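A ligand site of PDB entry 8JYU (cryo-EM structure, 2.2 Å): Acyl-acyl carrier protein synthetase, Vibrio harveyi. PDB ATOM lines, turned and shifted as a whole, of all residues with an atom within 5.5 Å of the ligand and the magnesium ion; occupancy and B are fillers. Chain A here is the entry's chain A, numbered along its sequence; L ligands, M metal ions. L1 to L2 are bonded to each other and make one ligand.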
ATOM      1  N   THR A 175      13.358 -18.812 -10.613  1.00  0.00           N
ATOM      2  CA  THR A 175      12.112 -19.096  -9.938  1.00  0.00           C
ATOM      3  C   THR A 175      10.968 -19.088 -10.940  1.00  0.00           C
ATOM      4  O   THR A 175      10.997 -18.347 -11.923  1.00  0.00           O
ATOM      5  CB  THR A 175      11.856 -18.081  -8.820  1.00  0.00           C
ATOM      6  OG1 THR A 175      10.656 -18.416  -8.115  1.00  0.00           O
ATOM      7  CG2 THR A 175      11.742 -16.669  -9.385  1.00  0.00           C
ATOM      8  N   ILE A 199      21.792 -14.598   9.621  1.00  0.00           N
ATOM      9  CA  ILE A 199      20.925 -15.638  10.139  1.00  0.00           C
ATOM     10  C   ILE A 199      21.601 -16.381  11.291  1.00  0.00           C
ATOM     11  O   ILE A 199      20.942 -16.734  12.277  1.00  0.00           O
ATOM     12  CB  ILE A 199      20.469 -16.604   9.024  1.00  0.00           C
ATOM     13  CG1 ILE A 199      19.332 -15.981   8.195  1.00  0.00           C
ATOM     14  CG2 ILE A 199      19.905 -17.865   9.622  1.00  0.00           C
ATOM     15  CD1 ILE A 199      19.717 -14.806   7.325  1.00  0.00           C
ATOM     16  N   HIS A 226      17.126 -25.155  -4.367  1.00  0.00           N
ATOM     17  CA  HIS A 226      16.062 -24.258  -3.932  1.00  0.00           C
ATOM     18  C   HIS A 226      16.663 -23.181  -3.036  1.00  0.00           C
ATOM     19  O   HIS A 226      16.775 -23.340  -1.817  1.00  0.00           O
ATOM     20  CB  HIS A 226      14.969 -25.044  -3.209  1.00  0.00           C
ATOM     21  CG  HIS A 226      13.748 -24.237  -2.906  1.00  0.00           C
ATOM     22  ND1 HIS A 226      13.272 -23.261  -3.751  1.00  0.00           N
ATOM     23  CD2 HIS A 226      12.901 -24.273  -1.851  1.00  0.00           C
ATOM     24  CE1 HIS A 226      12.181 -22.727  -3.234  1.00  0.00           C
ATOM     25  NE2 HIS A 226      11.940 -23.318  -2.071  1.00  0.00           N
ATOM     26  N   VAL A 227      17.039 -22.055  -3.654  1.00  0.00           N
ATOM     27  CA  VAL A 227      17.598 -20.888  -2.982  1.00  0.00           C
ATOM     28  C   VAL A 227      18.706 -21.280  -2.014  1.00  0.00           C
ATOM     29  O   VAL A 227      18.594 -21.058  -0.808  1.00  0.00           O
ATOM     30  CB  VAL A 227      16.500 -20.088  -2.249  1.00  0.00           C
ATOM     31  CG1 VAL A 227      15.886 -20.937  -1.155  1.00  0.00           C
ATOM     32  CG2 VAL A 227      17.069 -18.801  -1.650  1.00  0.00           C
ATOM     33  N   TRP A 230      18.079 -22.794   1.211  1.00  0.00           N
ATOM     34  CA  TRP A 230      17.794 -21.783   2.234  1.00  0.00           C
ATOM     35  C   TRP A 230      19.064 -21.268   2.904  1.00  0.00           C
ATOM     36  O   TRP A 230      19.010 -20.759   4.031  1.00  0.00           O
ATOM     37  CB  TRP A 230      16.792 -22.298   3.282  1.00  0.00           C
ATOM     38  CG  TRP A 230      15.510 -22.788   2.681  1.00  0.00           C
ATOM     39  CD1 TRP A 230      15.086 -22.622   1.392  1.00  0.00           C
ATOM     40  CD2 TRP A 230      14.483 -23.534   3.342  1.00  0.00           C
ATOM     41  NE1 TRP A 230      13.862 -23.215   1.214  1.00  0.00           N
ATOM     42  CE2 TRP A 230      13.468 -23.778   2.397  1.00  0.00           C
ATOM     43  CE3 TRP A 230      14.315 -24.015   4.649  1.00  0.00           C
ATOM     44  CZ2 TRP A 230      12.307 -24.479   2.719  1.00  0.00           C
ATOM     45  CZ3 TRP A 230      13.168 -24.711   4.955  1.00  0.00           C
ATOM     46  CH2 TRP A 230      12.175 -24.938   3.991  1.00  0.00           C
ATOM     47  N   LEU A 232      21.388 -22.705   4.343  1.00  0.00           N
ATOM     48  CA  LEU A 232      21.784 -23.454   5.533  1.00  0.00           C
ATOM     49  C   LEU A 232      23.011 -24.345   5.353  1.00  0.00           C
ATOM     50  O   LEU A 232      23.734 -24.552   6.329  1.00  0.00           O
ATOM     51  CB  LEU A 232      20.597 -24.281   6.026  1.00  0.00           C
ATOM     52  CG  LEU A 232      19.602 -23.420   6.821  1.00  0.00           C
ATOM     53  CD1 LEU A 232      18.185 -23.926   6.683  1.00  0.00           C
ATOM     54  CD2 LEU A 232      20.011 -23.347   8.275  1.00  0.00           C
ATOM     55  N   VAL A 293      12.951 -26.720  10.905  1.00  0.00           N
ATOM     56  CA  VAL A 293      12.361 -25.434  10.571  1.00  0.00           C
ATOM     57  C   VAL A 293      11.631 -25.564   9.246  1.00  0.00           C
ATOM     58  O   VAL A 293      12.197 -26.064   8.264  1.00  0.00           O
ATOM     59  CB  VAL A 293      13.423 -24.321  10.522  1.00  0.00           C
ATOM     60  CG1 VAL A 293      14.638 -24.752   9.732  1.00  0.00           C
ATOM     61  CG2 VAL A 293      12.830 -23.038   9.942  1.00  0.00           C
ATOM     62  N   ILE A 294      10.373 -25.140   9.219  1.00  0.00           N
ATOM     63  CA  ILE A 294       9.481 -25.361   8.083  1.00  0.00           C
ATOM     64  C   ILE A 294       9.342 -24.047   7.320  1.00  0.00           C
ATOM     65  O   ILE A 294       8.908 -23.036   7.882  1.00  0.00           O
ATOM     66  CB  ILE A 294       8.115 -25.877   8.549  1.00  0.00           C
ATOM     67  CG1 ILE A 294       8.280 -27.123   9.405  1.00  0.00           C
ATOM     68  CG2 ILE A 294       7.229 -26.170   7.356  1.00  0.00           C
ATOM     69  CD1 ILE A 294       8.935 -28.279   8.684  1.00  0.00           C
ATOM     70  N   GLY A 295       9.707 -24.085   6.036  1.00  0.00           N
ATOM     71  CA  GLY A 295       9.589 -22.911   5.179  1.00  0.00           C
ATOM     72  C   GLY A 295       9.014 -23.301   3.833  1.00  0.00           C
ATOM     73  O   GLY A 295       8.618 -24.445   3.605  1.00  0.00           O
ATOM     74  N   GLY A 296       8.962 -22.313   2.941  1.00  0.00           N
ATOM     75  CA  GLY A 296       8.441 -22.505   1.604  1.00  0.00           C
ATOM     76  C   GLY A 296       6.933 -22.469   1.487  1.00  0.00           C
ATOM     77  O   GLY A 296       6.419 -22.116   0.426  1.00  0.00           O
ATOM     78  N   ALA A 297       6.214 -22.824   2.544  1.00  0.00           N
ATOM     79  CA  ALA A 297       4.752 -22.786   2.541  1.00  0.00           C
ATOM     80  C   ALA A 297       4.267 -22.635   3.967  1.00  0.00           C
ATOM     81  O   ALA A 297       5.010 -22.860   4.923  1.00  0.00           O
ATOM     82  CB  ALA A 297       4.162 -24.052   1.897  1.00  0.00           C
ATOM     83  N   ALA A 298       3.001 -22.226   4.100  1.00  0.00           N
ATOM     84  CA  ALA A 298       2.424 -22.042   5.424  1.00  0.00           C
ATOM     85  C   ALA A 298       2.367 -23.369   6.170  1.00  0.00           C
ATOM     86  O   ALA A 298       1.924 -24.382   5.629  1.00  0.00           O
ATOM     87  CB  ALA A 298       1.016 -21.443   5.296  1.00  0.00           C
ATOM     88  N   LEU A 299       2.832 -23.350   7.413  1.00  0.00           N
ATOM     89  CA  LEU A 299       2.819 -24.562   8.230  1.00  0.00           C
ATOM     90  C   LEU A 299       1.448 -24.729   8.874  1.00  0.00           C
ATOM     91  O   LEU A 299       1.032 -23.853   9.655  1.00  0.00           O
ATOM     92  CB  LEU A 299       3.904 -24.484   9.293  1.00  0.00           C
ATOM     93  CG  LEU A 299       3.905 -25.568  10.370  1.00  0.00           C
ATOM     94  CD1 LEU A 299       4.103 -26.947   9.753  1.00  0.00           C
ATOM     95  CD2 LEU A 299       4.964 -25.285  11.417  1.00  0.00           C
ATOM     96  N   ALA A 316       8.526 -22.235  12.201  1.00  0.00           N
ATOM     97  CA  ALA A 316       8.380 -21.844  10.810  1.00  0.00           C
ATOM     98  C   ALA A 316       9.370 -20.743  10.429  1.00  0.00           C
ATOM     99  O   ALA A 316       9.916 -20.038  11.282  1.00  0.00           O
ATOM    100  CB  ALA A 316       6.960 -21.375  10.531  1.00  0.00           C
ATOM    101  N   GLY A 317       9.595 -20.623   9.128  1.00  0.00           N
ATOM    102  CA  GLY A 317      10.423 -19.568   8.568  1.00  0.00           C
ATOM    103  C   GLY A 317       9.837 -19.121   7.260  1.00  0.00           C
ATOM    104  O   GLY A 317       8.947 -19.771   6.702  1.00  0.00           O
ATOM    105  N   TYR A 318      10.351 -18.002   6.743  1.00  0.00           N
ATOM    106  CA  TYR A 318       9.779 -17.423   5.536  1.00  0.00           C
ATOM    107  C   TYR A 318      10.885 -16.836   4.666  1.00  0.00           C
ATOM    108  O   TYR A 318      11.861 -16.274   5.171  1.00  0.00           O
ATOM    109  CB  TYR A 318       8.743 -16.342   5.876  1.00  0.00           C
ATOM    110  CG  TYR A 318       8.396 -15.430   4.731  1.00  0.00           C
ATOM    111  CD1 TYR A 318       7.778 -15.912   3.591  1.00  0.00           C
ATOM    112  CD2 TYR A 318       8.682 -14.068   4.787  1.00  0.00           C
ATOM    113  CE1 TYR A 318       7.464 -15.087   2.534  1.00  0.00           C
ATOM    114  CE2 TYR A 318       8.366 -13.232   3.739  1.00  0.00           C
ATOM    115  CZ  TYR A 318       7.755 -13.745   2.616  1.00  0.00           C
ATOM    116  OH  TYR A 318       7.436 -12.915   1.575  1.00  0.00           O
ATOM    117  N   GLY A 319      10.706 -16.982   3.361  1.00  0.00           N
ATOM    118  CA  GLY A 319      11.623 -16.393   2.408  1.00  0.00           C
ATOM    119  C   GLY A 319      11.169 -16.722   0.997  1.00  0.00           C
ATOM    120  O   GLY A 319      10.173 -17.411   0.785  1.00  0.00           O
ATOM    121  N   MET A 320      11.935 -16.207   0.035  1.00  0.00           N
ATOM    122  CA  MET A 320      11.681 -16.499  -1.366  1.00  0.00           C
ATOM    123  C   MET A 320      13.003 -16.474  -2.118  1.00  0.00           C
ATOM    124  O   MET A 320      14.028 -16.019  -1.603  1.00  0.00           O
ATOM    125  CB  MET A 320      10.709 -15.513  -2.010  1.00  0.00           C
ATOM    126  CG  MET A 320      11.120 -14.073  -1.910  1.00  0.00           C
ATOM    127  SD  MET A 320       9.715 -12.953  -1.756  1.00  0.00           S
ATOM    128  CE  MET A 320       9.530 -12.482  -3.474  1.00  0.00           C
ATOM    129  N   SER A 321      12.960 -16.965  -3.361  1.00  0.00           N
ATOM    130  CA  SER A 321      14.141 -17.055  -4.207  1.00  0.00           C
ATOM    131  C   SER A 321      14.829 -15.705  -4.361  1.00  0.00           C
ATOM    132  O   SER A 321      16.056 -15.635  -4.532  1.00  0.00           O
ATOM    133  CB  SER A 321      13.777 -17.616  -5.574  1.00  0.00           C
ATOM    134  OG  SER A 321      13.308 -18.950  -5.473  1.00  0.00           O
ATOM    135  N   GLU A 322      14.057 -14.619  -4.309  1.00  0.00           N
ATOM    136  CA  GLU A 322      14.604 -13.290  -4.493  1.00  0.00           C
ATOM    137  C   GLU A 322      15.276 -12.723  -3.249  1.00  0.00           C
ATOM    138  O   GLU A 322      16.015 -11.737  -3.360  1.00  0.00           O
ATOM    139  CB  GLU A 322      13.499 -12.327  -4.936  1.00  0.00           C
ATOM    140  CG  GLU A 322      12.911 -12.605  -6.315  1.00  0.00           C
ATOM    141  CD  GLU A 322      11.852 -13.687  -6.294  1.00  0.00           C
ATOM    142  OE1 GLU A 322      11.656 -14.321  -5.231  1.00  0.00           O
ATOM    143  OE2 GLU A 322      11.213 -13.913  -7.340  1.00  0.00           O
ATOM    144  N   PRO A 325      17.217 -16.964   0.903  1.00  0.00           N
ATOM    145  CA  PRO A 325      15.828 -16.490   1.016  1.00  0.00           C
ATOM    146  C   PRO A 325      15.416 -15.921   2.369  1.00  0.00           C
ATOM    147  O   PRO A 325      14.450 -15.168   2.425  1.00  0.00           O
ATOM    148  CB  PRO A 325      15.042 -17.763   0.726  1.00  0.00           C
ATOM    149  CG  PRO A 325      15.859 -18.832   1.419  1.00  0.00           C
ATOM    150  CD  PRO A 325      17.306 -18.371   1.315  1.00  0.00           C
ATOM    151  N   ILE A 326      16.117 -16.245   3.457  1.00  0.00           N
ATOM    152  CA  ILE A 326      15.542 -16.096   4.794  1.00  0.00           C
ATOM    153  C   ILE A 326      15.256 -14.618   5.082  1.00  0.00           C
ATOM    154  O   ILE A 326      16.153 -13.774   5.007  1.00  0.00           O
ATOM    155  CB  ILE A 326      16.474 -16.694   5.850  1.00  0.00           C
ATOM    156  CG1 ILE A 326      16.707 -18.176   5.567  1.00  0.00           C
ATOM    157  CG2 ILE A 326      15.885 -16.513   7.236  1.00  0.00           C
ATOM    158  CD1 ILE A 326      17.782 -18.803   6.423  1.00  0.00           C
ATOM    159  N   SER A 328      12.384 -14.065   7.699  1.00  0.00           N
ATOM    160  CA  SER A 328      11.815 -14.125   9.041  1.00  0.00           C
ATOM    161  C   SER A 328      11.848 -15.563   9.528  1.00  0.00           C
ATOM    162  O   SER A 328      11.647 -16.503   8.759  1.00  0.00           O
ATOM    163  CB  SER A 328      10.387 -13.576   9.081  1.00  0.00           C
ATOM    164  OG  SER A 328       9.504 -14.406   8.349  1.00  0.00           O
ATOM    165  N   ILE A 329      12.107 -15.727  10.824  1.00  0.00           N
ATOM    166  CA  ILE A 329      12.133 -17.030  11.474  1.00  0.00           C
ATOM    167  C   ILE A 329      11.354 -16.934  12.785  1.00  0.00           C
ATOM    168  O   ILE A 329      11.434 -15.926  13.484  1.00  0.00           O
ATOM    169  CB  ILE A 329      13.571 -17.523  11.741  1.00  0.00           C
ATOM    170  CG1 ILE A 329      14.388 -17.540  10.441  1.00  0.00           C
ATOM    171  CG2 ILE A 329      13.570 -18.904  12.370  1.00  0.00           C
ATOM    172  CD1 ILE A 329      15.862 -17.789  10.667  1.00  0.00           C
ATOM    173  N   LYS A 350       3.375 -19.323  12.847  1.00  0.00           N
ATOM    174  CA  LYS A 350       3.379 -17.982  12.295  1.00  0.00           C
ATOM    175  C   LYS A 350       4.440 -17.861  11.214  1.00  0.00           C
ATOM    176  O   LYS A 350       5.348 -18.683  11.093  1.00  0.00           O
ATOM    177  CB  LYS A 350       3.642 -16.960  13.397  1.00  0.00           C
ATOM    178  CG  LYS A 350       2.578 -16.901  14.477  1.00  0.00           C
ATOM    179  CD  LYS A 350       1.472 -15.931  14.107  1.00  0.00           C
ATOM    180  CE  LYS A 350       0.559 -15.665  15.292  1.00  0.00           C
ATOM    181  NZ  LYS A 350      -0.169 -14.372  15.154  1.00  0.00           N
ATOM    182  N   THR A 351       4.309 -16.816  10.394  1.00  0.00           N
ATOM    183  CA  THR A 351       5.332 -16.525   9.398  1.00  0.00           C
ATOM    184  C   THR A 351       6.673 -16.191  10.041  1.00  0.00           C
ATOM    185  O   THR A 351       7.717 -16.499   9.463  1.00  0.00           O
ATOM    186  CB  THR A 351       4.858 -15.389   8.485  1.00  0.00           C
ATOM    187  OG1 THR A 351       3.586 -15.732   7.928  1.00  0.00           O
ATOM    188  CG2 THR A 351       5.836 -15.146   7.365  1.00  0.00           C
ATOM    189  N   THR A 409       7.507  -8.601  -2.154  1.00  0.00           N
ATOM    190  CA  THR A 409       7.436 -10.043  -1.993  1.00  0.00           C
ATOM    191  C   THR A 409       6.226 -10.659  -2.683  1.00  0.00           C
ATOM    192  O   THR A 409       6.246 -11.850  -3.010  1.00  0.00           O
ATOM    193  CB  THR A 409       7.413 -10.415  -0.514  1.00  0.00           C
ATOM    194  OG1 THR A 409       6.219  -9.910   0.089  1.00  0.00           O
ATOM    195  CG2 THR A 409       8.627  -9.836   0.202  1.00  0.00           C
ATOM    196  N   ASP A 411       3.445 -11.156  -1.166  1.00  0.00           N
ATOM    197  CA  ASP A 411       2.722 -11.845  -0.117  1.00  0.00           C
ATOM    198  C   ASP A 411       1.945 -10.835   0.721  1.00  0.00           C
ATOM    199  O   ASP A 411       2.482  -9.801   1.113  1.00  0.00           O
ATOM    200  CB  ASP A 411       3.664 -12.654   0.770  1.00  0.00           C
ATOM    201  CG  ASP A 411       4.430 -13.702   0.004  1.00  0.00           C
ATOM    202  OD1 ASP A 411       3.815 -14.407  -0.820  1.00  0.00           O
ATOM    203  OD2 ASP A 411       5.649 -13.823   0.213  1.00  0.00           O
ATOM    204  N   ILE A 423       1.315 -14.554   7.105  1.00  0.00           N
ATOM    205  CA  ILE A 423       0.933 -14.429   5.702  1.00  0.00           C
ATOM    206  C   ILE A 423      -0.491 -14.943   5.515  1.00  0.00           C
ATOM    207  O   ILE A 423      -0.833 -16.048   5.960  1.00  0.00           O
ATOM    208  CB  ILE A 423       1.922 -15.179   4.808  1.00  0.00           C
ATOM    209  CG1 ILE A 423       3.222 -14.396   4.671  1.00  0.00           C
ATOM    210  CG2 ILE A 423       1.319 -15.445   3.432  1.00  0.00           C
ATOM    211  CD1 ILE A 423       4.310 -15.157   3.979  1.00  0.00           C
ATOM    212  N   ARG A 426      -1.438 -14.571  -1.411  1.00  0.00           N
ATOM    213  CA  ARG A 426      -0.635 -13.826  -2.371  1.00  0.00           C
ATOM    214  C   ARG A 426      -1.367 -12.557  -2.800  1.00  0.00           C
ATOM    215  O   ARG A 426      -2.578 -12.404  -2.588  1.00  0.00           O
ATOM    216  CB  ARG A 426      -0.340 -14.687  -3.603  1.00  0.00           C
ATOM    217  CG  ARG A 426       0.500 -15.917  -3.318  1.00  0.00           C
ATOM    218  CD  ARG A 426       1.962 -15.559  -3.164  1.00  0.00           C
ATOM    219  NE  ARG A 426       2.543 -15.082  -4.415  1.00  0.00           N
ATOM    220  CZ  ARG A 426       3.716 -14.476  -4.514  1.00  0.00           C
ATOM    221  NH1 ARG A 426       4.477 -14.261  -3.459  1.00  0.00           N
ATOM    222  NH2 ARG A 426       4.134 -14.075  -5.714  1.00  0.00           N
ATOM    223  N   LYS A 522       2.406 -26.165  -6.905  1.00  0.00           N
ATOM    224  CA  LYS A 522       1.441 -25.202  -6.393  1.00  0.00           C
ATOM    225  C   LYS A 522       0.281 -25.045  -7.358  1.00  0.00           C
ATOM    226  O   LYS A 522       0.385 -25.331  -8.553  1.00  0.00           O
ATOM    227  CB  LYS A 522       2.106 -23.851  -6.151  1.00  0.00           C
ATOM    228  CG  LYS A 522       3.167 -23.867  -5.052  1.00  0.00           C
ATOM    229  CD  LYS A 522       3.845 -22.511  -4.922  1.00  0.00           C
ATOM    230  CE  LYS A 522       4.907 -22.538  -3.832  1.00  0.00           C
ATOM    231  NZ  LYS A 522       5.672 -21.262  -3.776  1.00  0.00           N
HETATM  232  P1  LIG L   1       9.946 -19.590  -3.820  1.00  0.00           P
HETATM  233  O1  LIG L   1      10.196 -18.353  -4.649  1.00  0.00           O
HETATM  234  O2  LIG L   1       9.855 -20.935  -4.503  1.00  0.00           O
HETATM  235  O3  LIG L   1       8.611 -19.359  -2.996  1.00  0.00           O
HETATM  236  C1  LIG L   1       8.394 -18.152  -2.286  1.00  0.00           C
HETATM  237  C2  LIG L   1       6.969 -18.011  -1.826  1.00  0.00           C
HETATM  238  O4  LIG L   1       6.647 -19.098  -0.927  1.00  0.00           O
HETATM  239  C3  LIG L   1       6.655 -16.766  -1.012  1.00  0.00           C
HETATM  240  O5  LIG L   1       6.465 -15.620  -1.812  1.00  0.00           O
HETATM  241  C4  LIG L   1       5.416 -17.179  -0.225  1.00  0.00           C
HETATM  242  O6  LIG L   1       4.254 -17.060  -1.034  1.00  0.00           O
HETATM  243  C5  LIG L   1       5.679 -18.670   0.020  1.00  0.00           C
HETATM  244  N1  LIG L   1       6.204 -18.926   1.369  1.00  0.00           N
HETATM  245  C6  LIG L   1       7.493 -19.132   1.695  1.00  0.00           C
HETATM  246  N2  LIG L   1       7.632 -19.328   3.028  1.00  0.00           N
HETATM  247  C7  LIG L   1       6.412 -19.253   3.577  1.00  0.00           C
HETATM  248  C8  LIG L   1       5.847 -19.367   4.944  1.00  0.00           C
HETATM  249  N3  LIG L   1       6.642 -19.612   6.011  1.00  0.00           N
HETATM  250  N4  LIG L   1       4.511 -19.216   5.081  1.00  0.00           N
HETATM  251  C9  LIG L   1       3.711 -18.966   4.030  1.00  0.00           C
HETATM  252  N5  LIG L   1       4.161 -18.853   2.768  1.00  0.00           N
HETATM  253  C10 LIG L   1       5.473 -18.982   2.478  1.00  0.00           C
HETATM  254  C1  LG2 L   2      10.709 -20.502  -1.372  1.00  0.00           C
HETATM  255  O1  LG2 L   2      10.699 -19.787  -2.473  1.00  0.00           O
HETATM  256  C2  LG2 L   2      11.711 -20.029  -0.365  1.00  0.00           C
HETATM  257  C3  LG2 L   2      11.549 -20.660   1.010  1.00  0.00           C
HETATM  258  C4  LG2 L   2      12.398 -19.986   2.071  1.00  0.00           C
HETATM  259  C5  LG2 L   2      12.227 -20.583   3.458  1.00  0.00           C
HETATM  260  C6  LG2 L   2      13.073 -19.916   4.527  1.00  0.00           C
HETATM  261  C7  LG2 L   2      12.871 -20.488   5.921  1.00  0.00           C
HETATM  262  C8  LG2 L   2      14.148 -21.002   6.569  1.00  0.00           C
HETATM  263  C9  LG2 L   2      14.433 -20.408   7.934  1.00  0.00           C
HETATM  264  C10 LG2 L   2      15.681 -20.972   8.570  1.00  0.00           C
HETATM  265  O2  LG2 L   2       9.978 -21.452  -1.188  1.00  0.00           O
HETATM  266 MG    MG M   1       9.708 -16.277  -5.306  1.00  0.00          MG
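Trp 230 touches the ligand.
Val 293 touches the ligand.
Gly 295 touches the ligand.
Ala 297 touches the ligand.
N of Ala 298 touches C9 of LIG L1, 3.3 Å away.
CD1 of Tyr 318 touches N2 of LIG L1, at 3.5 Å.
O of Gly 319 touches C2 of LG2 L2, 3.2 Å away.
CB of Met 320 touches C1 of LIG L1, 3.5 Å away.
Pro 325 touches the ligand.
CD1 of Ile 326 touches C10 of LG2 L2, at 3.7 Å.
CG1 of Ile 329 touches C9 of LG2 L2, at 3.8 Å.
O of Thr 409 touches O5 of LIG L1 (3.96 Å).
CD1 of Ile 423 touches C9 of LIG L1, 3.9 Å away.
NZ of Lys 522 touches O3 of LIG L1, 3.6 Å away.
Hydrophobic or aromatic side chains that line the ligand: His 226, Trp 230, Val 293, Ala 298, Tyr 318, Met 320, Pro 325, Ile 326, Ile 329 and Ile 423.
The nearest printed residue that does not touch the ligand is Leu 232 (4.3 Å).
Merely in contact with the magnesium ion: Met 320, Thr 175 and Ser 321.
Within 4 Å of the magnesium ion: Thr 175, Met 320, Ser 321 and Glu 322.
The nearest printed residue that does not touch the magnesium ion is Arg 426 (5.9 Å).
N of Gly 317 sits at hydrogen-bond distance from O of Ile 294 (2.8 Å).
The side-chain carboxylate (OD1) of Asp 411 lies within salt-bridge range of the guanidinium group (NH1) of Arg 426, 2.7 Å away.
OD2 of Asp 411 is in hydrogen-bond range of OH of Tyr 318 (2.4 Å).
N of Asp 411 lies close to OG1 of Thr 409 (3.3 Å).
The guanidinium group (NH1) of Arg 426 sits at hydrogen-bond distance from the backbone carbonyl oxygen (O) of Thr 409 (3.0 Å).
N of Tyr 318 sits at hydrogen-bond distance from O of Ser 328 (2.8 Å).
The backbone NH (N) of Ile 423 lies within hydrogen-bond range of the side-chain hydroxyl (OG1) of Thr 351.
A nitrogen (N3) of LIG L1 sits at hydrogen-bond distance from the backbone carbonyl oxygen of Gly 317, 2.4 Å away.
The side-chain carboxylate of Asp 411 lies within hydrogen-bond range of an oxygen (O6) of LIG L1.
An oxygen (O2) of LG2 L2 is in hydrogen-bond range of a ring nitrogen (NE2) of His 226 (2.8 Å).
The guanidinium group (NH1) of Arg 426 sits at hydrogen-bond distance from an oxygen (O5) of LIG L1 (2.9 Å).
A nitrogen (N2) of LIG L1 is in hydrogen-bond range of the backbone NH (N) of Gly 296, 3.3 Å away.
An oxygen (O1) of LIG L1 lies close to the backbone NH of Ser 321.
OG of Ser 321 lies close to O1 of LIG L1 (3.3 Å).
OG1 of Thr 175 lies close to O1 of LIG L1 (3.5 Å).
The magnesium ion is bound by an oxygen (O1) of LIG L1.
Slightly farther from the magnesium ion lies OE1 of Glu 322 (2.8 Å).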
